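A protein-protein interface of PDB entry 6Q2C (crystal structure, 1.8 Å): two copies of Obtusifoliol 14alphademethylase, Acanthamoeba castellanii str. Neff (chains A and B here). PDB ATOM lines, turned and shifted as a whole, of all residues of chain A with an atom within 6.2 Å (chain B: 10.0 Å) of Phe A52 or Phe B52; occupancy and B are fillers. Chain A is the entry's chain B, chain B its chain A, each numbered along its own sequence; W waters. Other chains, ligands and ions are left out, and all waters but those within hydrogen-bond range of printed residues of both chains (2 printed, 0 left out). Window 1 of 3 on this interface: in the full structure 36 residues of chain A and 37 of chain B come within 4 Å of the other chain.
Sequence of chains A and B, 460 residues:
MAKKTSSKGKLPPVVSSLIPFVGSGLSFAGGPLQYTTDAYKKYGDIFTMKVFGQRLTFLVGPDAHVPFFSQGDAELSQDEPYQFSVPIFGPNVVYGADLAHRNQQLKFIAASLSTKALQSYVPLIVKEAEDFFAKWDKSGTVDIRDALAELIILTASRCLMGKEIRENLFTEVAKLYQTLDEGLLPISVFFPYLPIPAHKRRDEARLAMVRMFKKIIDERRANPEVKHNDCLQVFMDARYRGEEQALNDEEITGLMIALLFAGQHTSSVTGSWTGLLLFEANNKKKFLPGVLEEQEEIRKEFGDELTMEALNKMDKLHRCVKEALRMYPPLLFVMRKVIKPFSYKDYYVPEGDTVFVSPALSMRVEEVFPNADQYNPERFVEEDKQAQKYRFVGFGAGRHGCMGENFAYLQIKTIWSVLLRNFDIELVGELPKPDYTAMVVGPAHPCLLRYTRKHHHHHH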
ATOM      1  N   LEU A  18     -17.558  11.960  -0.205  1.00  0.00           N
ATOM      2  CA  LEU A  18     -18.185  10.933   0.612  1.00  0.00           C
ATOM      3  C   LEU A  18     -17.128  10.067   1.252  1.00  0.00           C
ATOM      4  O   LEU A  18     -16.186   9.674   0.596  1.00  0.00           O
ATOM      5  CB  LEU A  18     -19.047  10.043  -0.295  1.00  0.00           C
ATOM      6  CG  LEU A  18     -20.195  10.742  -1.098  1.00  0.00           C
ATOM      7  CD1 LEU A  18     -20.820   9.857  -2.193  1.00  0.00           C
ATOM      8  CD2 LEU A  18     -21.255  11.214  -0.121  1.00  0.00           C
ATOM      9  N   ILE A  19     -17.304   9.729   2.528  1.00  0.00           N
ATOM     10  CA  ILE A  19     -16.374   8.832   3.238  1.00  0.00           C
ATOM     11  C   ILE A  19     -17.248   7.863   3.996  1.00  0.00           C
ATOM     12  O   ILE A  19     -17.591   8.135   5.146  1.00  0.00           O
ATOM     13  CB  ILE A  19     -15.466   9.614   4.216  1.00  0.00           C
ATOM     14  CG1 ILE A  19     -14.687  10.750   3.518  1.00  0.00           C
ATOM     15  CG2 ILE A  19     -14.506   8.655   4.894  1.00  0.00           C
ATOM     16  CD1 ILE A  19     -13.823  11.622   4.436  1.00  0.00           C
ATOM     17  N   PRO A  20     -17.690   6.772   3.355  1.00  0.00           N
ATOM     18  CA  PRO A  20     -18.617   5.944   4.140  1.00  0.00           C
ATOM     19  C   PRO A  20     -17.901   5.063   5.153  1.00  0.00           C
ATOM     20  O   PRO A  20     -16.671   4.860   5.108  1.00  0.00           O
ATOM     21  CB  PRO A  20     -19.254   5.047   3.104  1.00  0.00           C
ATOM     22  CG  PRO A  20     -18.221   4.882   2.079  1.00  0.00           C
ATOM     23  CD  PRO A  20     -17.550   6.267   1.987  1.00  0.00           C
ATOM     24  N   PHE A  21     -18.713   4.515   6.032  1.00  0.00           N
ATOM     25  CA  PHE A  21     -18.264   3.620   7.065  1.00  0.00           C
ATOM     26  C   PHE A  21     -17.874   2.332   6.391  1.00  0.00           C
ATOM     27  O   PHE A  21     -18.687   1.774   5.713  1.00  0.00           O
ATOM     28  CB  PHE A  21     -19.429   3.423   8.062  1.00  0.00           C
ATOM     29  CG  PHE A  21     -19.240   2.264   9.017  1.00  0.00           C
ATOM     30  CD1 PHE A  21     -18.378   2.367  10.088  1.00  0.00           C
ATOM     31  CD2 PHE A  21     -19.965   1.099   8.873  1.00  0.00           C
ATOM     32  CE1 PHE A  21     -18.247   1.329  10.993  1.00  0.00           C
ATOM     33  CE2 PHE A  21     -19.805   0.051   9.755  1.00  0.00           C
ATOM     34  CZ  PHE A  21     -18.920   0.153  10.795  1.00  0.00           C
ATOM     35  N   VAL A  22     -16.634   1.813   6.554  1.00  0.00           N
ATOM     36  CA  VAL A  22     -16.209   0.643   5.750  1.00  0.00           C
ATOM     37  C   VAL A  22     -16.511  -0.730   6.377  1.00  0.00           C
ATOM     38  O   VAL A  22     -16.594  -1.749   5.665  1.00  0.00           O
ATOM     39  CB  VAL A  22     -14.694   0.713   5.387  1.00  0.00           C
ATOM     40  CG1 VAL A  22     -13.833   0.270   6.528  1.00  0.00           C
ATOM     41  CG2 VAL A  22     -14.397  -0.191   4.196  1.00  0.00           C
ATOM     42  N   LYS A  50      -6.543  -2.013   8.916  1.00  0.00           N
ATOM     43  CA  LYS A  50      -6.927  -0.672   8.552  1.00  0.00           C
ATOM     44  C   LYS A  50      -7.215  -0.680   7.048  1.00  0.00           C
ATOM     45  O   LYS A  50      -6.436  -1.241   6.247  1.00  0.00           O
ATOM     46  CB  LYS A  50      -5.885   0.377   8.855  1.00  0.00           C
ATOM     47  CG  LYS A  50      -5.909   0.833  10.265  1.00  0.00           C
ATOM     48  CD  LYS A  50      -4.533   1.287  10.767  1.00  0.00           C
ATOM     49  CE  LYS A  50      -4.088   2.568  10.128  1.00  0.00           C
ATOM     50  NZ  LYS A  50      -5.020   3.682  10.297  1.00  0.00           N
ATOM     51  N   VAL A  51      -8.364  -0.095   6.710  1.00  0.00           N
ATOM     52  CA  VAL A  51      -8.835   0.030   5.313  1.00  0.00           C
ATOM     53  C   VAL A  51      -9.328   1.449   5.160  1.00  0.00           C
ATOM     54  O   VAL A  51     -10.153   1.904   5.941  1.00  0.00           O
ATOM     55  CB  VAL A  51      -9.910  -1.042   4.972  1.00  0.00           C
ATOM     56  CG1 VAL A  51     -10.373  -0.898   3.527  1.00  0.00           C
ATOM     57  CG2 VAL A  51      -9.362  -2.455   5.163  1.00  0.00           C
ATOM     58  N   PHE A  52      -8.777   2.202   4.194  1.00  0.00           N
ATOM     59  CA  PHE A  52      -9.071   3.612   4.082  1.00  0.00           C
ATOM     60  C   PHE A  52      -8.841   4.385   5.371  1.00  0.00           C
ATOM     61  O   PHE A  52      -9.502   5.366   5.674  1.00  0.00           O
ATOM     62  CB  PHE A  52     -10.500   3.840   3.523  1.00  0.00           C
ATOM     63  CG  PHE A  52     -10.726   3.223   2.179  1.00  0.00           C
ATOM     64  CD1 PHE A  52     -10.032   3.725   1.025  1.00  0.00           C
ATOM     65  CD2 PHE A  52     -11.608   2.168   2.007  1.00  0.00           C
ATOM     66  CE1 PHE A  52     -10.264   3.182  -0.254  1.00  0.00           C
ATOM     67  CE2 PHE A  52     -11.789   1.597   0.750  1.00  0.00           C
ATOM     68  CZ  PHE A  52     -11.104   2.102  -0.387  1.00  0.00           C
ATOM     69  N   GLY A  53      -7.839   3.965   6.127  1.00  0.00           N
ATOM     70  CA  GLY A  53      -7.556   4.626   7.350  1.00  0.00           C
ATOM     71  C   GLY A  53      -8.509   4.331   8.521  1.00  0.00           C
ATOM     72  O   GLY A  53      -8.322   4.931   9.552  1.00  0.00           O
ATOM     73  N   GLN A  54      -9.485   3.422   8.380  1.00  0.00           N
ATOM     74  CA  GLN A  54     -10.457   3.109   9.431  1.00  0.00           C
ATOM     75  C   GLN A  54     -10.008   1.829  10.061  1.00  0.00           C
ATOM     76  O   GLN A  54      -9.712   0.864   9.387  1.00  0.00           O
ATOM     77  CB  GLN A  54     -11.852   2.901   8.842  1.00  0.00           C
ATOM     78  CG  GLN A  54     -12.354   4.193   8.240  1.00  0.00           C
ATOM     79  CD  GLN A  54     -13.711   4.074   7.552  1.00  0.00           C
ATOM     80  OE1 GLN A  54     -14.584   3.312   7.968  1.00  0.00           O
ATOM     81  NE2 GLN A  54     -13.905   4.888   6.509  1.00  0.00           N
ATOM     82  N   PHE A 190     -22.824   0.720   2.145  1.00  0.00           N
ATOM     83  CA  PHE A 190     -22.118   1.974   2.103  1.00  0.00           C
ATOM     84  C   PHE A 190     -23.035   3.139   1.809  1.00  0.00           C
ATOM     85  O   PHE A 190     -22.889   4.193   2.407  1.00  0.00           O
ATOM     86  CB  PHE A 190     -21.014   1.845   1.013  1.00  0.00           C
ATOM     87  CG  PHE A 190     -20.044   0.695   1.274  1.00  0.00           C
ATOM     88  CD1 PHE A 190     -19.055   0.796   2.248  1.00  0.00           C
ATOM     89  CD2 PHE A 190     -20.177  -0.516   0.614  1.00  0.00           C
ATOM     90  CE1 PHE A 190     -18.145  -0.251   2.478  1.00  0.00           C
ATOM     91  CE2 PHE A 190     -19.309  -1.573   0.852  1.00  0.00           C
ATOM     92  CZ  PHE A 190     -18.299  -1.445   1.805  1.00  0.00           C
ATOM     93  N   SER B  16      -2.279  -5.157   8.824  1.00  0.00           N
ATOM     94  CA  SER B  16      -2.456  -4.752   7.441  1.00  0.00           C
ATOM     95  C   SER B  16      -3.022  -3.309   7.445  1.00  0.00           C
ATOM     96  O   SER B  16      -3.939  -3.010   8.199  1.00  0.00           O
ATOM     97  CB  SER B  16      -3.459  -5.752   6.836  1.00  0.00           C
ATOM     98  OG  SER B  16      -3.746  -5.468   5.502  1.00  0.00           O
ATOM     99  N   SER B  17      -2.445  -2.407   6.669  1.00  0.00           N
ATOM    100  CA  SER B  17      -3.078  -1.144   6.385  1.00  0.00           C
ATOM    101  C   SER B  17      -3.116  -1.002   4.852  1.00  0.00           C
ATOM    102  O   SER B  17      -2.066  -1.091   4.186  1.00  0.00           O
ATOM    103  CB  SER B  17      -2.339   0.037   6.976  1.00  0.00           C
ATOM    104  OG  SER B  17      -3.076   1.215   6.691  1.00  0.00           O
ATOM    105  N   LEU B  18      -4.313  -0.784   4.302  1.00  0.00           N
ATOM    106  CA  LEU B  18      -4.520  -0.743   2.866  1.00  0.00           C
ATOM    107  C   LEU B  18      -5.392   0.421   2.407  1.00  0.00           C
ATOM    108  O   LEU B  18      -6.395   0.803   3.059  1.00  0.00           O
ATOM    109  CB  LEU B  18      -5.043  -2.105   2.416  1.00  0.00           C
ATOM    110  CG  LEU B  18      -4.203  -3.367   2.705  1.00  0.00           C
ATOM    111  CD1 LEU B  18      -4.959  -4.658   2.436  1.00  0.00           C
ATOM    112  CD2 LEU B  18      -2.933  -3.349   1.836  1.00  0.00           C
ATOM    113  N   ILE B  19      -5.031   1.004   1.259  1.00  0.00           N
ATOM    114  CA  ILE B  19      -5.831   2.073   0.618  1.00  0.00           C
ATOM    115  C   ILE B  19      -5.930   1.686  -0.835  1.00  0.00           C
ATOM    116  O   ILE B  19      -5.051   1.975  -1.623  1.00  0.00           O
ATOM    117  CB  ILE B  19      -5.293   3.486   0.835  1.00  0.00           C
ATOM    118  CG1 ILE B  19      -5.169   3.791   2.325  1.00  0.00           C
ATOM    119  CG2 ILE B  19      -6.177   4.516   0.126  1.00  0.00           C
ATOM    120  CD1 ILE B  19      -4.631   5.168   2.658  1.00  0.00           C
ATOM    121  N   PRO B  20      -6.992   0.944  -1.194  1.00  0.00           N
ATOM    122  CA  PRO B  20      -7.054   0.497  -2.576  1.00  0.00           C
ATOM    123  C   PRO B  20      -7.662   1.627  -3.464  1.00  0.00           C
ATOM    124  O   PRO B  20      -8.229   2.630  -2.969  1.00  0.00           O
ATOM    125  CB  PRO B  20      -7.947  -0.745  -2.493  1.00  0.00           C
ATOM    126  CG  PRO B  20      -8.800  -0.529  -1.282  1.00  0.00           C
ATOM    127  CD  PRO B  20      -7.911   0.206  -0.299  1.00  0.00           C
ATOM    128  N   PHE B  21      -7.469   1.429  -4.762  1.00  0.00           N
ATOM    129  CA  PHE B  21      -8.027   2.221  -5.842  1.00  0.00           C
ATOM    130  C   PHE B  21      -9.531   1.966  -5.815  1.00  0.00           C
ATOM    131  O   PHE B  21      -9.913   0.805  -5.844  1.00  0.00           O
ATOM    132  CB  PHE B  21      -7.496   1.656  -7.159  1.00  0.00           C
ATOM    133  CG  PHE B  21      -8.081   2.313  -8.391  1.00  0.00           C
ATOM    134  CD1 PHE B  21      -7.801   3.653  -8.677  1.00  0.00           C
ATOM    135  CD2 PHE B  21      -8.834   1.583  -9.275  1.00  0.00           C
ATOM    136  CE1 PHE B  21      -8.282   4.250  -9.846  1.00  0.00           C
ATOM    137  CE2 PHE B  21      -9.303   2.173 -10.427  1.00  0.00           C
ATOM    138  CZ  PHE B  21      -9.043   3.510 -10.701  1.00  0.00           C
ATOM    139  N   VAL B  22     -10.340   3.020  -5.723  1.00  0.00           N
ATOM    140  CA  VAL B  22     -11.784   2.859  -5.536  1.00  0.00           C
ATOM    141  C   VAL B  22     -12.547   2.822  -6.872  1.00  0.00           C
ATOM    142  O   VAL B  22     -13.631   2.278  -6.936  1.00  0.00           O
ATOM    143  CB  VAL B  22     -12.315   3.950  -4.573  1.00  0.00           C
ATOM    144  CG1 VAL B  22     -12.633   5.214  -5.323  1.00  0.00           C
ATOM    145  CG2 VAL B  22     -13.549   3.484  -3.859  1.00  0.00           C
ATOM    146  N   GLY B  23     -11.995   3.459  -7.912  1.00  0.00           N
ATOM    147  CA  GLY B  23     -12.644   3.593  -9.219  1.00  0.00           C
ATOM    148  C   GLY B  23     -13.330   2.384  -9.854  1.00  0.00           C
ATOM    149  O   GLY B  23     -14.467   2.504 -10.386  1.00  0.00           O
ATOM    150  N   SER B  24     -12.720   1.208  -9.755  1.00  0.00           N
ATOM    151  CA  SER B  24     -13.328   0.033 -10.386  1.00  0.00           C
ATOM    152  C   SER B  24     -14.559  -0.491  -9.641  1.00  0.00           C
ATOM    153  O   SER B  24     -15.324  -1.246 -10.208  1.00  0.00           O
ATOM    154  CB  SER B  24     -12.347  -1.102 -10.721  1.00  0.00           C
ATOM    155  OG  SER B  24     -11.090  -0.876 -10.196  1.00  0.00           O
ATOM    156  N   GLY B  25     -14.787   0.006  -8.427  1.00  0.00           N
ATOM    157  CA  GLY B  25     -16.009  -0.221  -7.679  1.00  0.00           C
ATOM    158  C   GLY B  25     -17.273   0.265  -8.367  1.00  0.00           C
ATOM    159  O   GLY B  25     -18.378  -0.202  -8.063  1.00  0.00           O
ATOM    160  N   MET B  49     -16.735  13.385  -8.613  1.00  0.00           N
ATOM    161  CA  MET B  49     -17.197  12.891  -7.296  1.00  0.00           C
ATOM    162  C   MET B  49     -15.943  12.449  -6.514  1.00  0.00           C
ATOM    163  O   MET B  49     -15.038  11.859  -7.119  1.00  0.00           O
ATOM    164  CB  MET B  49     -18.067  11.652  -7.453  1.00  0.00           C
ATOM    165  CG  MET B  49     -19.340  11.802  -8.304  1.00  0.00           C
ATOM    166  SD  MET B  49     -20.181  10.209  -8.678  1.00  0.00           S
ATOM    167  CE  MET B  49     -21.602  10.892  -9.549  1.00  0.00           C
ATOM    168  N   LYS B  50     -15.890  12.699  -5.198  1.00  0.00           N
ATOM    169  CA  LYS B  50     -14.779  12.202  -4.381  1.00  0.00           C
ATOM    170  C   LYS B  50     -15.367  11.121  -3.478  1.00  0.00           C
ATOM    171  O   LYS B  50     -16.449  11.288  -2.863  1.00  0.00           O
ATOM    172  CB  LYS B  50     -14.070  13.272  -3.514  1.00  0.00           C
ATOM    173  CG  LYS B  50     -13.334  14.412  -4.213  1.00  0.00           C
ATOM    174  CD  LYS B  50     -12.543  15.276  -3.178  1.00  0.00           C
ATOM    175  CE  LYS B  50     -12.470  16.772  -3.459  1.00  0.00           C
ATOM    176  NZ  LYS B  50     -11.298  17.304  -4.241  1.00  0.00           N
ATOM    177  N   VAL B  51     -14.659  10.007  -3.411  1.00  0.00           N
ATOM    178  CA  VAL B  51     -14.974   8.910  -2.519  1.00  0.00           C
ATOM    179  C   VAL B  51     -13.640   8.499  -1.832  1.00  0.00           C
ATOM    180  O   VAL B  51     -12.701   8.144  -2.512  1.00  0.00           O
ATOM    181  CB  VAL B  51     -15.525   7.720  -3.296  1.00  0.00           C
ATOM    182  CG1 VAL B  51     -15.881   6.617  -2.363  1.00  0.00           C
ATOM    183  CG2 VAL B  51     -16.762   8.185  -4.102  1.00  0.00           C
ATOM    184  N   PHE B  52     -13.626   8.451  -0.500  1.00  0.00           N
ATOM    185  CA  PHE B  52     -12.408   8.303   0.312  1.00  0.00           C
ATOM    186  C   PHE B  52     -11.290   9.254  -0.136  1.00  0.00           C
ATOM    187  O   PHE B  52     -10.113   8.894  -0.238  1.00  0.00           O
ATOM    188  CB  PHE B  52     -11.940   6.863   0.262  1.00  0.00           C
ATOM    189  CG  PHE B  52     -12.930   5.863   0.795  1.00  0.00           C
ATOM    190  CD1 PHE B  52     -13.355   5.898   2.126  1.00  0.00           C
ATOM    191  CD2 PHE B  52     -13.414   4.828  -0.003  1.00  0.00           C
ATOM    192  CE1 PHE B  52     -14.244   4.914   2.637  1.00  0.00           C
ATOM    193  CE2 PHE B  52     -14.333   3.886   0.501  1.00  0.00           C
ATOM    194  CZ  PHE B  52     -14.725   3.925   1.835  1.00  0.00           C
ATOM    195  N   GLY B  53     -11.685  10.417  -0.578  1.00  0.00           N
ATOM    196  CA  GLY B  53     -10.752  11.413  -1.044  1.00  0.00           C
ATOM    197  C   GLY B  53     -10.218  11.214  -2.442  1.00  0.00           C
ATOM    198  O   GLY B  53      -9.491  12.041  -2.867  1.00  0.00           O
ATOM    199  N   GLN B  54     -10.606  10.131  -3.145  1.00  0.00           N
ATOM    200  CA  GLN B  54     -10.127   9.846  -4.514  1.00  0.00           C
ATOM    201  C   GLN B  54     -11.060  10.565  -5.471  1.00  0.00           C
ATOM    202  O   GLN B  54     -12.306  10.469  -5.354  1.00  0.00           O
ATOM    203  CB  GLN B  54     -10.122   8.363  -4.795  1.00  0.00           C
ATOM    204  CG  GLN B  54      -9.158   7.653  -3.831  1.00  0.00           C
ATOM    205  CD  GLN B  54      -9.018   6.178  -4.073  1.00  0.00           C
ATOM    206  OE1 GLN B  54      -9.135   5.678  -5.210  1.00  0.00           O
ATOM    207  NE2 GLN B  54      -8.669   5.436  -2.990  1.00  0.00           N
ATOM    208  N   ARG B  55     -10.478  11.280  -6.402  1.00  0.00           N
ATOM    209  CA  ARG B  55     -11.288  12.093  -7.331  1.00  0.00           C
ATOM    210  C   ARG B  55     -11.691  11.265  -8.542  1.00  0.00           C
ATOM    211  O   ARG B  55     -10.831  10.764  -9.274  1.00  0.00           O
ATOM    212  CB  ARG B  55     -10.477  13.349  -7.753  1.00  0.00           C
ATOM    213  CG  ARG B  55     -10.266  14.333  -6.614  1.00  0.00           C
ATOM    214  CD  ARG B  55      -9.173  15.387  -6.909  1.00  0.00           C
ATOM    215  NE  ARG B  55      -9.391  15.920  -8.239  1.00  0.00           N
ATOM    216  CZ  ARG B  55     -10.257  16.839  -8.616  1.00  0.00           C
ATOM    217  NH1 ARG B  55     -10.986  17.523  -7.759  1.00  0.00           N
ATOM    218  NH2 ARG B  55     -10.378  17.101  -9.920  1.00  0.00           N
ATOM    219  N   LEU B  56     -13.004  11.199  -8.838  1.00  0.00           N
ATOM    220  CA  LEU B  56     -13.544  10.474  -9.980  1.00  0.00           C
ATOM    221  C   LEU B  56     -14.226  11.491 -10.892  1.00  0.00           C
ATOM    222  O   LEU B  56     -15.221  12.120 -10.502  1.00  0.00           O
ATOM    223  CB  LEU B  56     -14.536   9.441  -9.480  1.00  0.00           C
ATOM    224  CG  LEU B  56     -14.023   8.537  -8.323  1.00  0.00           C
ATOM    225  CD1 LEU B  56     -15.205   7.657  -7.880  1.00  0.00           C
ATOM    226  CD2 LEU B  56     -12.801   7.738  -8.754  1.00  0.00           C
ATOM    227  N   ILE B 187     -15.727  -7.615  -4.220  1.00  0.00           N
ATOM    228  CA  ILE B 187     -14.498  -7.435  -3.402  1.00  0.00           C
ATOM    229  C   ILE B 187     -13.185  -7.614  -4.253  1.00  0.00           C
ATOM    230  O   ILE B 187     -12.153  -6.981  -3.956  1.00  0.00           O
ATOM    231  CB  ILE B 187     -14.448  -8.414  -2.228  1.00  0.00           C
ATOM    232  CG1 ILE B 187     -13.309  -8.051  -1.257  1.00  0.00           C
ATOM    233  CG2 ILE B 187     -14.282  -9.843  -2.704  1.00  0.00           C
ATOM    234  CD1 ILE B 187     -13.529  -6.797  -0.463  1.00  0.00           C
ATOM    235  N   VAL B 189     -12.408  -6.487  -7.116  1.00  0.00           N
ATOM    236  CA  VAL B 189     -11.913  -5.289  -7.822  1.00  0.00           C
ATOM    237  C   VAL B 189     -11.116  -4.362  -6.886  1.00  0.00           C
ATOM    238  O   VAL B 189     -10.429  -3.480  -7.362  1.00  0.00           O
ATOM    239  CB  VAL B 189     -13.011  -4.529  -8.581  1.00  0.00           C
ATOM    240  CG1 VAL B 189     -13.773  -5.501  -9.479  1.00  0.00           C
ATOM    241  CG2 VAL B 189     -13.955  -3.789  -7.634  1.00  0.00           C
ATOM    242  N   PHE B 190     -11.213  -4.572  -5.585  1.00  0.00           N
ATOM    243  CA  PHE B 190     -10.441  -3.812  -4.581  1.00  0.00           C
ATOM    244  C   PHE B 190      -9.248  -4.625  -4.134  1.00  0.00           C
ATOM    245  O   PHE B 190      -8.147  -4.097  -4.053  1.00  0.00           O
ATOM    246  CB  PHE B 190     -11.263  -3.460  -3.387  1.00  0.00           C
ATOM    247  CG  PHE B 190     -12.437  -2.601  -3.720  1.00  0.00           C
ATOM    248  CD1 PHE B 190     -12.311  -1.256  -3.925  1.00  0.00           C
ATOM    249  CD2 PHE B 190     -13.702  -3.158  -3.832  1.00  0.00           C
ATOM    250  CE1 PHE B 190     -13.420  -0.452  -4.244  1.00  0.00           C
ATOM    251  CE2 PHE B 190     -14.820  -2.375  -4.174  1.00  0.00           C
ATOM    252  CZ  PHE B 190     -14.673  -1.021  -4.380  1.00  0.00           C
ATOM    253  N   PHE B 191      -9.477  -5.898  -3.884  1.00  0.00           N
ATOM    254  CA  PHE B 191      -8.449  -6.838  -3.431  1.00  0.00           C
ATOM    255  C   PHE B 191      -8.362  -8.114  -4.245  1.00  0.00           C
ATOM    256  O   PHE B 191      -8.890  -9.153  -3.840  1.00  0.00           O
ATOM    257  CB  PHE B 191      -8.672  -7.173  -1.966  1.00  0.00           C
ATOM    258  CG  PHE B 191      -8.735  -5.984  -1.088  1.00  0.00           C
ATOM    259  CD1 PHE B 191      -7.600  -5.198  -0.897  1.00  0.00           C
ATOM    260  CD2 PHE B 191      -9.920  -5.597  -0.486  1.00  0.00           C
ATOM    261  CE1 PHE B 191      -7.681  -4.064  -0.109  1.00  0.00           C
ATOM    262  CE2 PHE B 191      -9.984  -4.493   0.325  1.00  0.00           C
ATOM    263  CZ  PHE B 191      -8.864  -3.746   0.545  1.00  0.00           C
HETATM  264  O   HOH W   1      -5.635   2.182   5.641  1.00  0.00           O
HETATM  265  O   HOH W   2     -14.215  11.789  -0.273  1.00  0.00           O
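Val B51 touches Leu A18. Pro A20 touches Phe B52 (O to CE1, 3.5 Å). Ser B17 touches Lys A50 (CA to O, 3.4 Å). O of Leu B18 touches CA of Val A51, 3.4 Å away. Pro B20 touches Phe A52 (O to CE1, 3.4 Å). Phe A52 touches Phe B52. CE1 of Phe A52 touches NE2 of Gln B54, at 3.9 Å. Phe B52 touches Gln A54 (CE1 to NE2, 3.9 Å).
O of Pro B20 sits at hydrogen-bond distance from NE2 of Gln B54, at 2.8 Å. The backbone NH of Val B22 lies within hydrogen-bond range of the side-chain amide oxygen of Gln B54, at 3.0 Å. The backbone carbonyl oxygen of Pro A20 sits at hydrogen-bond distance from the side-chain amide nitrogen of Gln A54 (3.1 Å). The side-chain amide oxygen (OE1) of Gln A54 lies within hydrogen-bond range of the backbone NH (N) of Val A22 (2.9 Å).
Leu A18 touches Lys B50, and with the chains exchanged Lys A50 touches Leu B18. Leu A18 touches Val B51, and with the chains exchanged Val A51 touches Leu B18. Phe A52 touches its own counterpart, Phe B52. Phe A52 touches Gln B54, and with the chains exchanged Gln A54 touches Phe B52. 11 positions are printed for both chains.
Water W1 lies within hydrogen-bond range of the backbone NH of Gly A53, the side-chain hydroxyl of Ser B17, the backbone carbonyl oxygen of Leu B18 and the backbone NH of Phe A52. Water W2 lies within hydrogen-bond range of N of Gly B53 (2.9 Å), O of Leu A18 (3.0 Å), N of Phe B52 (3.4 Å) and O of Lys B50 (3.5 Å).
Of the 11 printed residues of chain A, 6 touch a printed residue of chain B. Among the printed residues, no Asp or Glu carboxylate lies within 4 Å of a Lys or Arg side-chain nitrogen of the other chain.
N of Leu B18 is in hydrogen-bond range of O of Lys A50, at 2.9 Å. N of Phe B52 sits at hydrogen-bond distance from O of Leu A18 (3.0 Å). The backbone carbonyl oxygen (O) of Ser B16 sits at hydrogen-bond distance from the backbone NH (N) of Lys A50 (2.9 Å). N of Phe A52 sits at hydrogen-bond distance from O of Leu B18. The backbone carbonyl oxygen of Lys B50 lies within hydrogen-bond range of the backbone NH of Leu A18 (3.0 Å).
Phe A52 touches just these residues of chain B: Leu B18 (3.0 Å), Pro B20 (3.4 Å), Phe B52 (3.4 Å) and Gln B54 (3.9 Å). Phe B52 touches just these residues of chain A: Leu A18 (3.0 Å), Pro A20 (3.5 Å), Phe A52 (3.4 Å) and Gln A54 (3.9 Å). No residue of chain B comes within 4 Å of Ile A19. Printed residues of chain B within 4 Å of Val A51: Leu B18. No residue of chain B comes within 4 Å of Gly A53. Gln A54 touches just one residue of chain B: Phe B52. Of the printed residues of chain B, Leu A18 touches Lys B50 (3.0 Å), Val B51 (3.4 Å) and Phe B52 (3.0 Å). Of the printed residues of chain A, Ser B17 touches Lys A50. Printed residues of chain A within 4 Å of Val B51: Leu A18 (3.4 Å). The nearest residue of chain A that does not touch Phe B52 is Ile A19 (4.1 Å). The nearest printed residue of chain A that does not touch Val B51 is Pro A20 (4.7 Å).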
